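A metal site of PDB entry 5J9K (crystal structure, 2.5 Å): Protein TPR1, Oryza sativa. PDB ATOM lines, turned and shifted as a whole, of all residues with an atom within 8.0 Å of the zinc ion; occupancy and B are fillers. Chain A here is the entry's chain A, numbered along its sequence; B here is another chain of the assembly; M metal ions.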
ATOM      1  N   LEU A 179      -5.233 -18.198  10.209  1.00  0.00           N
ATOM      2  CA  LEU A 179      -4.895 -19.589  10.465  1.00  0.00           C
ATOM      3  C   LEU A 179      -4.509 -19.750  11.932  1.00  0.00           C
ATOM      4  O   LEU A 179      -4.886 -20.725  12.583  1.00  0.00           O
ATOM      5  CB  LEU A 179      -3.777 -20.038   9.523  1.00  0.00           C
ATOM      6  CG  LEU A 179      -4.262 -20.035   8.077  1.00  0.00           C
ATOM      7  CD1 LEU A 179      -3.147 -20.381   7.099  1.00  0.00           C
ATOM      8  CD2 LEU A 179      -5.476 -20.949   7.892  1.00  0.00           C
ATOM      9  N   ASN A 180      -3.793 -18.764  12.454  1.00  0.00           N
ATOM     10  CA  ASN A 180      -3.455 -18.726  13.870  1.00  0.00           C
ATOM     11  C   ASN A 180      -4.703 -18.648  14.743  1.00  0.00           C
ATOM     12  O   ASN A 180      -4.791 -19.323  15.763  1.00  0.00           O
ATOM     13  CB  ASN A 180      -2.526 -17.551  14.162  1.00  0.00           C
ATOM     14  CG  ASN A 180      -1.054 -17.925  14.016  1.00  0.00           C
ATOM     15  OD1 ASN A 180      -0.230 -17.571  14.851  1.00  0.00           O
ATOM     16  ND2 ASN A 180      -0.723 -18.641  12.960  1.00  0.00           N
ATOM     17  N   TRP A 181      -5.669 -17.847  14.333  1.00  0.00           N
ATOM     18  CA  TRP A 181      -6.897 -17.741  15.097  1.00  0.00           C
ATOM     19  C   TRP A 181      -7.644 -19.076  15.123  1.00  0.00           C
ATOM     20  O   TRP A 181      -8.076 -19.522  16.185  1.00  0.00           O
ATOM     21  CB  TRP A 181      -7.811 -16.641  14.559  1.00  0.00           C
ATOM     22  CG  TRP A 181      -8.921 -16.364  15.520  1.00  0.00           C
ATOM     23  CD1 TRP A 181      -8.845 -15.664  16.695  1.00  0.00           C
ATOM     24  CD2 TRP A 181     -10.275 -16.818  15.416  1.00  0.00           C
ATOM     25  NE1 TRP A 181     -10.074 -15.641  17.325  1.00  0.00           N
ATOM     26  CE2 TRP A 181     -10.964 -16.352  16.554  1.00  0.00           C
ATOM     27  CE3 TRP A 181     -10.965 -17.581  14.471  1.00  0.00           C
ATOM     28  CZ2 TRP A 181     -12.316 -16.607  16.766  1.00  0.00           C
ATOM     29  CZ3 TRP A 181     -12.317 -17.836  14.683  1.00  0.00           C
ATOM     30  CH2 TRP A 181     -12.972 -17.346  15.825  1.00  0.00           C
ATOM     31  N   GLN A 182      -7.789 -19.704  13.961  1.00  0.00           N
ATOM     32  CA  GLN A 182      -8.483 -20.988  13.882  1.00  0.00           C
ATOM     33  C   GLN A 182      -7.822 -22.077  14.721  1.00  0.00           C
ATOM     34  O   GLN A 182      -8.513 -22.837  15.418  1.00  0.00           O
ATOM     35  CB  GLN A 182      -8.567 -21.446  12.436  1.00  0.00           C
ATOM     36  CG  GLN A 182      -9.369 -20.550  11.572  1.00  0.00           C
ATOM     37  CD  GLN A 182      -9.238 -20.873  10.111  1.00  0.00           C
ATOM     38  OE1 GLN A 182      -9.120 -22.040   9.726  1.00  0.00           O
ATOM     39  NE2 GLN A 182      -9.253 -19.843   9.277  1.00  0.00           N
ATOM     40  N   HIS A 183      -6.505 -22.151  14.649  1.00  0.00           N
ATOM     41  CA  HIS A 183      -5.765 -23.213  15.313  1.00  0.00           C
ATOM     42  C   HIS A 183      -5.758 -23.061  16.825  1.00  0.00           C
ATOM     43  O   HIS A 183      -5.789 -24.034  17.562  1.00  0.00           O
ATOM     44  CB  HIS A 183      -4.320 -23.258  14.805  1.00  0.00           C
ATOM     45  CG  HIS A 183      -3.450 -24.207  15.548  1.00  0.00           C
ATOM     46  ND1 HIS A 183      -3.563 -25.578  15.421  1.00  0.00           N
ATOM     47  CD2 HIS A 183      -2.469 -23.990  16.450  1.00  0.00           C
ATOM     48  CE1 HIS A 183      -2.671 -26.161  16.199  1.00  0.00           C
ATOM     49  NE2 HIS A 183      -1.987 -25.221  16.836  1.00  0.00           N
ATOM     50  N   GLN A 184      -5.723 -21.808  17.259  1.00  0.00           N
ATOM     51  CA  GLN A 184      -5.761 -21.452  18.670  1.00  0.00           C
ATOM     52  C   GLN A 184      -7.102 -21.860  19.329  1.00  0.00           C
ATOM     53  O   GLN A 184      -7.205 -21.951  20.553  1.00  0.00           O
ATOM     54  CB  GLN A 184      -5.481 -19.947  18.805  1.00  0.00           C
ATOM     55  CG  GLN A 184      -5.922 -19.280  20.085  1.00  0.00           C
ATOM     56  CD  GLN A 184      -7.175 -18.463  19.888  1.00  0.00           C
ATOM     57  OE1 GLN A 184      -7.859 -18.584  18.861  1.00  0.00           O
ATOM     58  NE2 GLN A 184      -7.480 -17.606  20.852  1.00  0.00           N
ATOM     59  N   LEU A 185      -8.095 -22.145  18.493  1.00  0.00           N
ATOM     60  CA  LEU A 185      -9.388 -22.659  18.968  1.00  0.00           C
ATOM     61  C   LEU A 185      -9.443 -24.179  19.018  1.00  0.00           C
ATOM     62  O   LEU A 185     -10.434 -24.752  19.465  1.00  0.00           O
ATOM     63  CB  LEU A 185     -10.509 -22.148  18.067  1.00  0.00           C
ATOM     64  CG  LEU A 185     -10.715 -20.641  18.025  1.00  0.00           C
ATOM     65  CD1 LEU A 185     -11.776 -20.338  17.007  1.00  0.00           C
ATOM     66  CD2 LEU A 185     -11.104 -20.115  19.391  1.00  0.00           C
ATOM     67  N   CYS A 186      -8.385 -24.843  18.545  1.00  0.00           N
ATOM     68  CA  CYS A 186      -8.331 -26.296  18.592  1.00  0.00           C
ATOM     69  C   CYS A 186      -8.045 -26.751  20.007  1.00  0.00           C
ATOM     70  O   CYS A 186      -7.614 -25.955  20.836  1.00  0.00           O
ATOM     71  CB  CYS A 186      -7.277 -26.834  17.634  1.00  0.00           C
ATOM     72  SG  CYS A 186      -7.550 -26.340  15.918  1.00  0.00           S
ATOM     73  N   LYS A 187      -8.298 -28.027  20.286  1.00  0.00           N
ATOM     74  CA  LYS A 187      -8.081 -28.556  21.627  1.00  0.00           C
ATOM     75  C   LYS A 187      -7.082 -29.704  21.620  1.00  0.00           C
ATOM     76  O   LYS A 187      -7.198 -30.650  22.401  1.00  0.00           O
ATOM     77  CB  LYS A 187      -9.406 -29.011  22.242  1.00  0.00           C
ATOM     78  CG  LYS A 187      -9.551 -28.608  23.703  1.00  0.00           C
ATOM     79  CD  LYS A 187      -9.311 -27.114  23.870  1.00  0.00           C
ATOM     80  CE  LYS A 187      -8.070 -26.818  24.698  1.00  0.00           C
ATOM     81  NZ  LYS A 187      -8.328 -26.936  26.166  1.00  0.00           N
ATOM     82  N   ASN A 188      -6.099 -29.613  20.727  1.00  0.00           N
ATOM     83  CA  ASN A 188      -5.054 -30.612  20.629  1.00  0.00           C
ATOM     84  C   ASN A 188      -3.742 -30.013  20.111  1.00  0.00           C
ATOM     85  O   ASN A 188      -3.748 -28.946  19.482  1.00  0.00           O
ATOM     86  CB  ASN A 188      -5.525 -31.759  19.708  1.00  0.00           C
ATOM     87  N   PRO A 189      -2.611 -30.671  20.398  1.00  0.00           N
ATOM     88  CA  PRO A 189      -1.317 -30.347  19.774  1.00  0.00           C
ATOM     89  C   PRO A 189      -1.357 -30.700  18.267  1.00  0.00           C
ATOM     90  O   PRO A 189      -2.358 -31.276  17.837  1.00  0.00           O
ATOM     91  CB  PRO A 189      -0.329 -31.220  20.567  1.00  0.00           C
ATOM     92  CG  PRO A 189      -1.149 -32.337  21.106  1.00  0.00           C
ATOM     93  CD  PRO A 189      -2.454 -31.701  21.447  1.00  0.00           C
ATOM     94  N   ARG A 190      -0.331 -30.367  17.471  1.00  0.00           N
ATOM     95  CA  ARG A 190       0.907 -29.718  17.910  1.00  0.00           C
ATOM     96  C   ARG A 190       1.417 -28.776  16.838  1.00  0.00           C
ATOM     97  O   ARG A 190       0.986 -28.859  15.697  1.00  0.00           O
ATOM     98  CB  ARG A 190       1.980 -30.772  18.219  1.00  0.00           C
ATOM     99  N   PRO A 191       2.339 -27.879  17.218  1.00  0.00           N
ATOM    100  CA  PRO A 191       3.013 -27.075  16.193  1.00  0.00           C
ATOM    101  C   PRO A 191       3.574 -27.955  15.068  1.00  0.00           C
ATOM    102  O   PRO A 191       3.892 -29.133  15.284  1.00  0.00           O
ATOM    103  CB  PRO A 191       4.124 -26.361  16.978  1.00  0.00           C
ATOM    104  CG  PRO A 191       4.130 -26.987  18.333  1.00  0.00           C
ATOM    105  CD  PRO A 191       2.732 -27.447  18.561  1.00  0.00           C
ATOM    106  N   PRO A 193       1.126 -27.959  12.777  1.00  0.00           N
ATOM    107  CA  PRO A 193      -0.167 -28.597  12.489  1.00  0.00           C
ATOM    108  C   PRO A 193      -0.536 -28.476  11.010  1.00  0.00           C
ATOM    109  O   PRO A 193      -0.070 -27.562  10.337  1.00  0.00           O
ATOM    110  CB  PRO A 193      -1.151 -27.828  13.383  1.00  0.00           C
ATOM    111  CG  PRO A 193      -0.573 -26.501  13.493  1.00  0.00           C
ATOM    112  CD  PRO A 193       0.926 -26.600  13.338  1.00  0.00           C
ATOM    113  N   ASP A 194      -1.311 -29.426  10.502  1.00  0.00           N
ATOM    114  CA  ASP A 194      -1.642 -29.470   9.083  1.00  0.00           C
ATOM    115  C   ASP A 194      -2.837 -28.587   8.753  1.00  0.00           C
ATOM    116  O   ASP A 194      -3.900 -28.696   9.369  1.00  0.00           O
ATOM    117  CB  ASP A 194      -1.917 -30.913   8.643  1.00  0.00           C
ATOM    118  CG  ASP A 194      -0.784 -31.857   9.026  1.00  0.00           C
ATOM    119  OD1 ASP A 194       0.359 -31.377   9.205  1.00  0.00           O
ATOM    120  OD2 ASP A 194      -1.030 -33.073   9.154  1.00  0.00           O
ATOM    121  N   ILE A 195      -2.651 -27.675   7.803  1.00  0.00           N
ATOM    122  CA  ILE A 195      -3.755 -26.864   7.345  1.00  0.00           C
ATOM    123  C   ILE A 195      -4.195 -27.346   5.984  1.00  0.00           C
ATOM    124  O   ILE A 195      -3.464 -27.272   5.004  1.00  0.00           O
ATOM    125  CB  ILE A 195      -3.378 -25.386   7.290  1.00  0.00           C
ATOM    126  CG1 ILE A 195      -3.020 -24.920   8.695  1.00  0.00           C
ATOM    127  CG2 ILE A 195      -4.525 -24.573   6.722  1.00  0.00           C
ATOM    128  CD1 ILE A 195      -2.832 -23.449   8.788  1.00  0.00           C
ATOM    129  N   HIS A 202      -9.895 -24.547   9.904  1.00  0.00           N
ATOM    130  CA  HIS A 202      -9.046 -25.660  10.300  1.00  0.00           C
ATOM    131  C   HIS A 202      -9.408 -26.195  11.686  1.00  0.00           C
ATOM    132  O   HIS A 202      -9.797 -25.424  12.564  1.00  0.00           O
ATOM    133  CB  HIS A 202      -7.575 -25.236  10.295  1.00  0.00           C
ATOM    134  CG  HIS A 202      -6.736 -25.937  11.327  1.00  0.00           C
ATOM    135  ND1 HIS A 202      -6.044 -27.092  11.054  1.00  0.00           N
ATOM    136  CD2 HIS A 202      -6.490 -25.650  12.625  1.00  0.00           C
ATOM    137  CE1 HIS A 202      -5.399 -27.483  12.136  1.00  0.00           C
ATOM    138  NE2 HIS A 202      -5.662 -26.625  13.107  1.00  0.00           N
ATOM    139  N   THR A 203      -9.294 -27.512  11.874  1.00  0.00           N
ATOM    140  CA  THR A 203      -9.420 -28.112  13.204  1.00  0.00           C
ATOM    141  C   THR A 203      -8.336 -29.176  13.438  1.00  0.00           C
ATOM    142  O   THR A 203      -7.757 -29.714  12.498  1.00  0.00           O
ATOM    143  CB  THR A 203     -10.800 -28.775  13.433  1.00  0.00           C
ATOM    144  OG1 THR A 203     -10.951 -29.904  12.553  1.00  0.00           O
ATOM    145  CG2 THR A 203     -11.929 -27.791  13.184  1.00  0.00           C
ATOM    146  N   CYS A 204      -8.078 -29.472  14.708  1.00  0.00           N
ATOM    147  CA  CYS A 204      -7.210 -30.583  15.071  1.00  0.00           C
ATOM    148  C   CYS A 204      -8.029 -31.662  15.784  1.00  0.00           C
ATOM    149  O   CYS A 204      -8.499 -31.451  16.894  1.00  0.00           O
ATOM    150  CB  CYS A 204      -6.064 -30.122  15.978  1.00  0.00           C
ATOM    151  SG  CYS A 204      -4.554 -29.587  15.119  1.00  0.00           S
ATOM    152  N   THR A 205      -8.201 -32.806  15.108  1.00  0.00           N
ATOM    153  CA  THR A 205      -8.865 -33.973  15.684  1.00  0.00           C
ATOM    154  C   THR A 205      -8.776 -35.136  14.715  1.00  0.00           C
ATOM    155  O   THR A 205      -8.501 -34.948  13.531  1.00  0.00           O
ATOM    156  CB  THR A 205     -10.328 -33.668  16.020  1.00  0.00           C
ATOM    157  N   TYR B   5       2.374 -21.948   6.886  1.00  0.00           N
ATOM    158  CA  TYR B   5       1.812 -21.548   8.152  1.00  0.00           C
ATOM    159  C   TYR B   5       2.897 -21.142   9.144  1.00  0.00           C
ATOM    160  O   TYR B   5       3.617 -21.988   9.666  1.00  0.00           O
ATOM    161  CB  TYR B   5       0.960 -22.682   8.721  1.00  0.00           C
ATOM    162  CG  TYR B   5       0.493 -22.457  10.133  1.00  0.00           C
ATOM    163  CD1 TYR B   5      -0.539 -21.568  10.411  1.00  0.00           C
ATOM    164  CD2 TYR B   5       1.082 -23.131  11.192  1.00  0.00           C
ATOM    165  CE1 TYR B   5      -0.975 -21.365  11.712  1.00  0.00           C
ATOM    166  CE2 TYR B   5       0.660 -22.927  12.493  1.00  0.00           C
ATOM    167  CZ  TYR B   5      -0.373 -22.047  12.748  1.00  0.00           C
ATOM    168  OH  TYR B   5      -0.812 -21.826  14.034  1.00  0.00           O
HETATM  169 ZN    ZN M   1      -5.216 -26.872  15.323  1.00  0.00          ZN
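A ring nitrogen (ND1) of His 183 is bound to the zinc ion (2.1 Å). The zinc ion is bound by NE2 of His 202 (2.3 Å). The zinc ion is bound by the side-chain sulfur (SG) of Cys 186, 2.5 Å away. Slightly farther from the zinc ion lies SG of Cys 204 (2.8 Å).
The nearest printed residue that does not touch the zinc ion is Thr 203 (4.3 Å).
A ring nitrogen (NE2) of His 202 sits close to the side-chain sulfur (SG) of Cys 204 (3.7 Å). N of His 202 lies within hydrogen-bond range of OE1 of Gln 182 (2.6 Å). A ring nitrogen (ND1) of His 202 is in hydrogen-bond range of the backbone carbonyl oxygen of Asp 194, 3.2 Å away. The side-chain sulfur (SG) of Cys 186 sits close to the backbone NH (N) of Cys 204 (3.4 Å). O of Gln 182 sits close to SG of Cys 186 (3.7 Å).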
